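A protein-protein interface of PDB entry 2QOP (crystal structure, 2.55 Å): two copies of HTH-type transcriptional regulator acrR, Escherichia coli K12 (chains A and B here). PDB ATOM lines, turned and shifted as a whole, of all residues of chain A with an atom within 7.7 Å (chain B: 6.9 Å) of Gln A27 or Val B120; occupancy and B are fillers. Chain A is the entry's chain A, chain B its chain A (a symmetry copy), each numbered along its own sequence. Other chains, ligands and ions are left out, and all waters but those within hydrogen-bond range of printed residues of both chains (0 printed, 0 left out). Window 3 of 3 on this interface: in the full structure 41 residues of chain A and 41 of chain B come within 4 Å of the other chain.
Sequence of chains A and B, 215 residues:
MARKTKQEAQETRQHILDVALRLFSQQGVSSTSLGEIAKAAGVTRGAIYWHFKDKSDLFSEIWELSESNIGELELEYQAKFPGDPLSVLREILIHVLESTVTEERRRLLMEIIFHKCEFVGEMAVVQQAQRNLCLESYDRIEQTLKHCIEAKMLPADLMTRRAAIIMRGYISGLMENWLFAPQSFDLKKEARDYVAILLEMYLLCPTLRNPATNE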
ATOM      1  N   ARG A  22      17.791  10.773 -17.444  1.00  0.00           N
ATOM      2  CA  ARG A  22      18.261  11.154 -18.773  1.00  0.00           C
ATOM      3  C   ARG A  22      18.938  12.525 -18.731  1.00  0.00           C
ATOM      4  O   ARG A  22      20.020  12.701 -19.290  1.00  0.00           O
ATOM      5  CB  ARG A  22      17.094  11.169 -19.764  1.00  0.00           C
ATOM      6  CG  ARG A  22      17.478  10.862 -21.205  1.00  0.00           C
ATOM      7  CD  ARG A  22      16.278  10.977 -22.144  1.00  0.00           C
ATOM      8  NE  ARG A  22      15.146  10.154 -21.715  1.00  0.00           N
ATOM      9  CZ  ARG A  22      13.987  10.060 -22.363  1.00  0.00           C
ATOM     10  NH1 ARG A  22      13.787  10.733 -23.489  1.00  0.00           N
ATOM     11  NH2 ARG A  22      13.023   9.286 -21.885  1.00  0.00           N
ATOM     12  N   LEU A  23      18.301  13.481 -18.058  1.00  0.00           N
ATOM     13  CA  LEU A  23      18.809  14.853 -17.968  1.00  0.00           C
ATOM     14  C   LEU A  23      20.016  15.005 -17.042  1.00  0.00           C
ATOM     15  O   LEU A  23      20.865  15.870 -17.269  1.00  0.00           O
ATOM     16  CB  LEU A  23      17.701  15.822 -17.543  1.00  0.00           C
ATOM     17  CG  LEU A  23      16.686  16.266 -18.601  1.00  0.00           C
ATOM     18  CD1 LEU A  23      15.520  16.972 -17.936  1.00  0.00           C
ATOM     19  CD2 LEU A  23      17.322  17.164 -19.659  1.00  0.00           C
ATOM     20  N   PHE A  24      20.086  14.172 -16.005  1.00  0.00           N
ATOM     21  CA  PHE A  24      21.208  14.206 -15.061  1.00  0.00           C
ATOM     22  C   PHE A  24      22.514  13.693 -15.674  1.00  0.00           C
ATOM     23  O   PHE A  24      23.583  13.844 -15.080  1.00  0.00           O
ATOM     24  CB  PHE A  24      20.882  13.432 -13.774  1.00  0.00           C
ATOM     25  CG  PHE A  24      19.846  14.093 -12.898  1.00  0.00           C
ATOM     26  CD1 PHE A  24      18.911  13.324 -12.210  1.00  0.00           C
ATOM     27  CD2 PHE A  24      19.804  15.479 -12.753  1.00  0.00           C
ATOM     28  CE1 PHE A  24      17.950  13.921 -11.397  1.00  0.00           C
ATOM     29  CE2 PHE A  24      18.847  16.086 -11.942  1.00  0.00           C
ATOM     30  CZ  PHE A  24      17.919  15.305 -11.263  1.00  0.00           C
ATOM     31  N   SER A  25      22.423  13.084 -16.855  1.00  0.00           N
ATOM     32  CA  SER A  25      23.597  12.567 -17.558  1.00  0.00           C
ATOM     33  C   SER A  25      24.173  13.573 -18.555  1.00  0.00           C
ATOM     34  O   SER A  25      25.390  13.641 -18.737  1.00  0.00           O
ATOM     35  CB  SER A  25      23.273  11.245 -18.260  1.00  0.00           C
ATOM     36  OG  SER A  25      22.306  11.425 -19.280  1.00  0.00           O
ATOM     37  N   GLN A  26      23.298  14.348 -19.195  1.00  0.00           N
ATOM     38  CA  GLN A  26      23.720  15.352 -20.173  1.00  0.00           C
ATOM     39  C   GLN A  26      24.317  16.604 -19.527  1.00  0.00           C
ATOM     40  O   GLN A  26      25.364  17.088 -19.960  1.00  0.00           O
ATOM     41  CB  GLN A  26      22.565  15.745 -21.104  1.00  0.00           C
ATOM     42  CG  GLN A  26      22.289  14.757 -22.232  1.00  0.00           C
ATOM     43  CD  GLN A  26      21.110  13.845 -21.948  1.00  0.00           C
ATOM     44  OE1 GLN A  26      19.984  14.308 -21.755  1.00  0.00           O
ATOM     45  NE2 GLN A  26      21.361  12.541 -21.937  1.00  0.00           N
ATOM     46  N   GLN A  27      23.647  17.119 -18.497  1.00  0.00           N
ATOM     47  CA  GLN A  27      24.048  18.380 -17.862  1.00  0.00           C
ATOM     48  C   GLN A  27      24.286  18.279 -16.349  1.00  0.00           C
ATOM     49  O   GLN A  27      24.482  19.296 -15.676  1.00  0.00           O
ATOM     50  CB  GLN A  27      23.041  19.494 -18.187  1.00  0.00           C
ATOM     51  CG  GLN A  27      21.583  19.155 -17.877  1.00  0.00           C
ATOM     52  CD  GLN A  27      20.629  20.296 -18.188  1.00  0.00           C
ATOM     53  OE1 GLN A  27      19.666  20.126 -18.935  1.00  0.00           O
ATOM     54  NE2 GLN A  27      20.894  21.467 -17.615  1.00  0.00           N
ATOM     55  N   GLY A  28      24.277  17.055 -15.822  1.00  0.00           N
ATOM     56  CA  GLY A  28      24.562  16.818 -14.407  1.00  0.00           C
ATOM     57  C   GLY A  28      23.381  17.059 -13.487  1.00  0.00           C
ATOM     58  O   GLY A  28      22.262  17.298 -13.945  1.00  0.00           O
ATOM     59  N   VAL A  29      23.642  16.995 -12.183  1.00  0.00           N
ATOM     60  CA  VAL A  29      22.612  17.198 -11.161  1.00  0.00           C
ATOM     61  C   VAL A  29      22.744  18.586 -10.528  1.00  0.00           C
ATOM     62  O   VAL A  29      21.761  19.153 -10.043  1.00  0.00           O
ATOM     63  CB  VAL A  29      22.672  16.102 -10.059  1.00  0.00           C
ATOM     64  CG1 VAL A  29      21.412  16.125  -9.200  1.00  0.00           C
ATOM     65  CG2 VAL A  29      22.856  14.720 -10.676  1.00  0.00           C
ATOM     66  N   SER A  30      23.962  19.127 -10.551  1.00  0.00           N
ATOM     67  CA  SER A  30      24.270  20.427  -9.952  1.00  0.00           C
ATOM     68  C   SER A  30      23.543  21.594 -10.621  1.00  0.00           C
ATOM     69  O   SER A  30      23.106  22.528  -9.944  1.00  0.00           O
ATOM     70  CB  SER A  30      25.781  20.677  -9.964  1.00  0.00           C
ATOM     71  OG  SER A  30      26.294  20.657 -11.286  1.00  0.00           O
ATOM     72  N   SER A  31      23.418  21.535 -11.945  1.00  0.00           N
ATOM     73  CA  SER A  31      22.794  22.609 -12.716  1.00  0.00           C
ATOM     74  C   SER A  31      21.426  22.219 -13.287  1.00  0.00           C
ATOM     75  O   SER A  31      20.962  22.809 -14.267  1.00  0.00           O
ATOM     76  CB  SER A  31      23.734  23.075 -13.835  1.00  0.00           C
ATOM     77  OG  SER A  31      24.040  22.013 -14.723  1.00  0.00           O
ATOM     78  N   THR A  32      20.785  21.232 -12.664  1.00  0.00           N
ATOM     79  CA  THR A  32      19.472  20.762 -13.104  1.00  0.00           C
ATOM     80  C   THR A  32      18.506  20.649 -11.924  1.00  0.00           C
ATOM     81  O   THR A  32      18.615  19.738 -11.100  1.00  0.00           O
ATOM     82  CB  THR A  32      19.566  19.408 -13.848  1.00  0.00           C
ATOM     83  OG1 THR A  32      20.733  19.390 -14.678  1.00  0.00           O
ATOM     84  CG2 THR A  32      18.332  19.181 -14.711  1.00  0.00           C
ATOM     85  N   SER A  33      17.568  21.590 -11.856  1.00  0.00           N
ATOM     86  CA  SER A  33      16.554  21.614 -10.804  1.00  0.00           C
ATOM     87  C   SER A  33      15.325  20.795 -11.201  1.00  0.00           C
ATOM     88  O   SER A  33      15.239  20.302 -12.328  1.00  0.00           O
ATOM     89  CB  SER A  33      16.157  23.058 -10.478  1.00  0.00           C
ATOM     90  OG  SER A  33      15.642  23.720 -11.621  1.00  0.00           O
ATOM     91  N   GLU A  36      13.419  22.013 -14.281  1.00  0.00           N
ATOM     92  CA  GLU A  36      13.982  21.622 -15.573  1.00  0.00           C
ATOM     93  C   GLU A  36      13.510  20.231 -15.991  1.00  0.00           C
ATOM     94  O   GLU A  36      13.383  19.944 -17.183  1.00  0.00           O
ATOM     95  CB  GLU A  36      15.512  21.676 -15.537  1.00  0.00           C
ATOM     96  CG  GLU A  36      16.087  23.089 -15.462  1.00  0.00           C
ATOM     97  CD  GLU A  36      17.606  23.113 -15.441  1.00  0.00           C
ATOM     98  OE1 GLU A  36      18.236  22.373 -16.229  1.00  0.00           O
ATOM     99  OE2 GLU A  36      18.173  23.886 -14.641  1.00  0.00           O
ATOM    100  N   ILE A  37      13.257  19.376 -15.002  1.00  0.00           N
ATOM    101  CA  ILE A  37      12.716  18.035 -15.235  1.00  0.00           C
ATOM    102  C   ILE A  37      11.226  18.116 -15.580  1.00  0.00           C
ATOM    103  O   ILE A  37      10.710  17.281 -16.329  1.00  0.00           O
ATOM    104  CB  ILE A  37      12.915  17.101 -13.998  1.00  0.00           C
ATOM    105  CG1 ILE A  37      14.310  17.274 -13.367  1.00  0.00           C
ATOM    106  CG2 ILE A  37      12.621  15.636 -14.354  1.00  0.00           C
ATOM    107  CD1 ILE A  37      15.481  16.742 -14.191  1.00  0.00           C
ATOM    108  N   HIS A 115      30.360   9.599 -12.521  1.00  0.00           N
ATOM    109  CA  HIS A 115      30.804  10.755 -13.307  1.00  0.00           C
ATOM    110  C   HIS A 115      29.986  12.034 -13.098  1.00  0.00           C
ATOM    111  O   HIS A 115      30.551  13.095 -12.827  1.00  0.00           O
ATOM    112  CB  HIS A 115      30.864  10.403 -14.801  1.00  0.00           C
ATOM    113  CG  HIS A 115      31.606   9.137 -15.098  1.00  0.00           C
ATOM    114  ND1 HIS A 115      32.970   9.016 -14.934  1.00  0.00           N
ATOM    115  CD2 HIS A 115      31.175   7.936 -15.550  1.00  0.00           C
ATOM    116  CE1 HIS A 115      33.345   7.795 -15.268  1.00  0.00           C
ATOM    117  NE2 HIS A 115      32.275   7.119 -15.647  1.00  0.00           N
ATOM    118  N   LYS A 116      28.663  11.929 -13.222  1.00  0.00           N
ATOM    119  CA  LYS A 116      27.792  13.109 -13.263  1.00  0.00           C
ATOM    120  C   LYS A 116      27.041  13.359 -11.949  1.00  0.00           C
ATOM    121  O   LYS A 116      25.819  13.536 -11.947  1.00  0.00           O
ATOM    122  CB  LYS A 116      26.796  12.999 -14.432  1.00  0.00           C
ATOM    123  CG  LYS A 116      27.362  12.422 -15.731  1.00  0.00           C
ATOM    124  CD  LYS A 116      28.215  13.427 -16.498  1.00  0.00           C
ATOM    125  CE  LYS A 116      28.869  12.785 -17.715  1.00  0.00           C
ATOM    126  NZ  LYS A 116      27.889  12.422 -18.779  1.00  0.00           N
ATOM    127  N   CYS A 117      27.775  13.385 -10.837  1.00  0.00           N
ATOM    128  CA  CYS A 117      27.170  13.580  -9.516  1.00  0.00           C
ATOM    129  C   CYS A 117      27.883  14.652  -8.687  1.00  0.00           C
ATOM    130  O   CYS A 117      29.041  14.982  -8.947  1.00  0.00           O
ATOM    131  CB  CYS A 117      27.132  12.258  -8.746  1.00  0.00           C
ATOM    132  SG  CYS A 117      26.057  12.267  -7.296  1.00  0.00           S
ATOM    133  N   CYS B 117      33.407  15.699  -8.684  1.00  0.00           N
ATOM    134  CA  CYS B 117      33.685  16.291  -9.996  1.00  0.00           C
ATOM    135  C   CYS B 117      32.416  16.559 -10.809  1.00  0.00           C
ATOM    136  O   CYS B 117      31.367  15.966 -10.552  1.00  0.00           O
ATOM    137  CB  CYS B 117      34.643  15.400 -10.791  1.00  0.00           C
ATOM    138  SG  CYS B 117      35.383  16.196 -12.232  1.00  0.00           S
ATOM    139  N   GLU B 118      32.530  17.453 -11.790  1.00  0.00           N
ATOM    140  CA  GLU B 118      31.408  17.820 -12.655  1.00  0.00           C
ATOM    141  C   GLU B 118      31.266  16.874 -13.847  1.00  0.00           C
ATOM    142  O   GLU B 118      30.246  16.195 -13.988  1.00  0.00           O
ATOM    143  CB  GLU B 118      31.557  19.260 -13.159  1.00  0.00           C
ATOM    144  CG  GLU B 118      31.426  20.339 -12.097  1.00  0.00           C
ATOM    145  CD  GLU B 118      31.404  21.737 -12.690  1.00  0.00           C
ATOM    146  OE1 GLU B 118      32.333  22.520 -12.399  1.00  0.00           O
ATOM    147  OE2 GLU B 118      30.467  22.050 -13.454  1.00  0.00           O
ATOM    148  N   PHE B 119      32.299  16.844 -14.692  1.00  0.00           N
ATOM    149  CA  PHE B 119      32.309  16.093 -15.959  1.00  0.00           C
ATOM    150  C   PHE B 119      31.165  16.472 -16.913  1.00  0.00           C
ATOM    151  O   PHE B 119      30.621  15.613 -17.610  1.00  0.00           O
ATOM    152  CB  PHE B 119      32.330  14.573 -15.715  1.00  0.00           C
ATOM    153  CG  PHE B 119      33.632  14.055 -15.165  1.00  0.00           C
ATOM    154  CD1 PHE B 119      33.664  13.369 -13.954  1.00  0.00           C
ATOM    155  CD2 PHE B 119      34.825  14.240 -15.859  1.00  0.00           C
ATOM    156  CE1 PHE B 119      34.864  12.879 -13.443  1.00  0.00           C
ATOM    157  CE2 PHE B 119      36.030  13.756 -15.354  1.00  0.00           C
ATOM    158  CZ  PHE B 119      36.049  13.075 -14.143  1.00  0.00           C
ATOM    159  N   VAL B 120      30.812  17.758 -16.950  1.00  0.00           N
ATOM    160  CA  VAL B 120      29.689  18.218 -17.780  1.00  0.00           C
ATOM    161  C   VAL B 120      30.039  19.329 -18.778  1.00  0.00           C
ATOM    162  O   VAL B 120      30.054  19.093 -19.988  1.00  0.00           O
ATOM    163  CB  VAL B 120      28.428  18.584 -16.934  1.00  0.00           C
ATOM    164  CG1 VAL B 120      27.692  17.322 -16.512  1.00  0.00           C
ATOM    165  CG2 VAL B 120      28.792  19.433 -15.716  1.00  0.00           C
ATOM    166  N   GLY B 121      30.317  20.530 -18.271  1.00  0.00           N
ATOM    167  CA  GLY B 121      30.569  21.696 -19.118  1.00  0.00           C
ATOM    168  C   GLY B 121      32.025  21.838 -19.513  1.00  0.00           C
ATOM    169  O   GLY B 121      32.493  21.165 -20.434  1.00  0.00           O
ATOM    170  N   GLU B 122      32.736  22.721 -18.815  1.00  0.00           N
ATOM    171  CA  GLU B 122      34.169  22.923 -19.032  1.00  0.00           C
ATOM    172  C   GLU B 122      34.992  21.769 -18.462  1.00  0.00           C
ATOM    173  O   GLU B 122      36.183  21.635 -18.759  1.00  0.00           O
ATOM    174  CB  GLU B 122      34.626  24.253 -18.420  1.00  0.00           C
ATOM    175  CG  GLU B 122      34.207  25.494 -19.206  1.00  0.00           C
ATOM    176  CD  GLU B 122      34.971  25.668 -20.512  1.00  0.00           C
ATOM    177  OE1 GLU B 122      34.369  26.161 -21.489  1.00  0.00           O
ATOM    178  OE2 GLU B 122      36.170  25.315 -20.565  1.00  0.00           O
ATOM    179  N   MET B 123      34.345  20.937 -17.648  1.00  0.00           N
ATOM    180  CA  MET B 123      34.981  19.776 -17.034  1.00  0.00           C
ATOM    181  C   MET B 123      34.930  18.552 -17.954  1.00  0.00           C
ATOM    182  O   MET B 123      35.450  17.486 -17.615  1.00  0.00           O
ATOM    183  CB  MET B 123      34.316  19.466 -15.690  1.00  0.00           C
ATOM    184  CG  MET B 123      35.276  18.995 -14.610  1.00  0.00           C
ATOM    185  SD  MET B 123      36.327  20.322 -13.986  1.00  0.00           S
ATOM    186  CE  MET B 123      37.185  19.479 -12.661  1.00  0.00           C
ATOM    187  N   ALA B 124      34.296  18.714 -19.114  1.00  0.00           N
ATOM    188  CA  ALA B 124      34.274  17.681 -20.146  1.00  0.00           C
ATOM    189  C   ALA B 124      35.546  17.733 -20.990  1.00  0.00           C
ATOM    190  O   ALA B 124      35.904  16.754 -21.649  1.00  0.00           O
ATOM    191  CB  ALA B 124      33.043  17.831 -21.025  1.00  0.00           C
ATOM    192  N   VAL B 125      36.218  18.884 -20.961  1.00  0.00           N
ATOM    193  CA  VAL B 125      37.479  19.089 -21.677  1.00  0.00           C
ATOM    194  C   VAL B 125      38.602  18.274 -21.030  1.00  0.00           C
ATOM    195  O   VAL B 125      39.392  17.632 -21.728  1.00  0.00           O
ATOM    196  CB  VAL B 125      37.871  20.593 -21.735  1.00  0.00           C
ATOM    197  CG1 VAL B 125      39.089  20.804 -22.630  1.00  0.00           C
ATOM    198  CG2 VAL B 125      36.703  21.440 -22.228  1.00  0.00           C
ATOM    199  N   GLN B 127      38.028  15.699 -19.165  1.00  0.00           N
ATOM    200  CA  GLN B 127      37.580  14.314 -19.319  1.00  0.00           C
ATOM    201  C   GLN B 127      38.124  13.723 -20.620  1.00  0.00           C
ATOM    202  O   GLN B 127      38.497  12.549 -20.668  1.00  0.00           O
ATOM    203  CB  GLN B 127      36.050  14.232 -19.291  1.00  0.00           C
ATOM    204  CG  GLN B 127      35.492  12.812 -19.185  1.00  0.00           C
ATOM    205  CD  GLN B 127      33.983  12.772 -18.998  1.00  0.00           C
ATOM    206  OE1 GLN B 127      33.475  12.068 -18.125  1.00  0.00           O
ATOM    207  NE2 GLN B 127      33.259  13.526 -19.821  1.00  0.00           N
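Cys B117 touches its own counterpart, Cys A117.
Position printed for both chains: 117.
Of the 8 pairs that touch across the chains among the printed residues, 1 has its exchanged pair printed and touching as well.
Gln A27 touches just one residue of chain B: Val B120.
No residue of chain A comes within 4 Å of Gly B121.
Of the printed residues of chain A, Phe B119 touches His A115 and Lys A116.
Of the printed residues of chain A, Glu B118 touches His A115 (3.3 Å).
Of the printed residues of chain B, His A115 touches Cys B117, Glu B118 and Phe B119.
Of the printed residues of chain B, Gly A28 touches Val B120 (3.5 Å).
Printed residues of chain A within 4 Å of Cys B117: His A115 and Cys A117.
Leu A23 touches none of the printed residues of chain B.
Of the 17 printed residues of chain A, 5 touch a printed residue of chain B.
Among the printed residues, 8 pairs touch across the chains.
Among the printed residues, no Asp or Glu carboxylate lies within 4 Å of a Lys or Arg side-chain nitrogen of the other chain.
Among the printed residues, merely in contact across the chains: Gln A27 with Val B120, Gly A28 with Val B120, His A115 with Cys B117, His A115 with Phe B119, Lys A116 with Phe B119 and Lys A116 with Val B120.
The backbone carbonyl oxygen of His A115 lies close to the backbone carbonyl oxygen of Glu B118, at 3.3 Å.
The backbone carbonyl oxygen (O) of Cys A117 sits close to the backbone carbonyl oxygen (O) of Cys B117.
O of Ser A25 sits at hydrogen-bond distance from NZ of Lys A116, at 2.8 Å.
O of Gln A27 is in hydrogen-bond range of OG of Ser A31 (2.9 Å).
NE2 of Gln A27 lies within hydrogen-bond range of OE1 of Glu A36, at 3.1 Å.
The backbone carbonyl oxygen (O) of Gly A28 sits at hydrogen-bond distance from the side-chain hydroxyl (OG1) of Thr A32 (2.7 Å).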
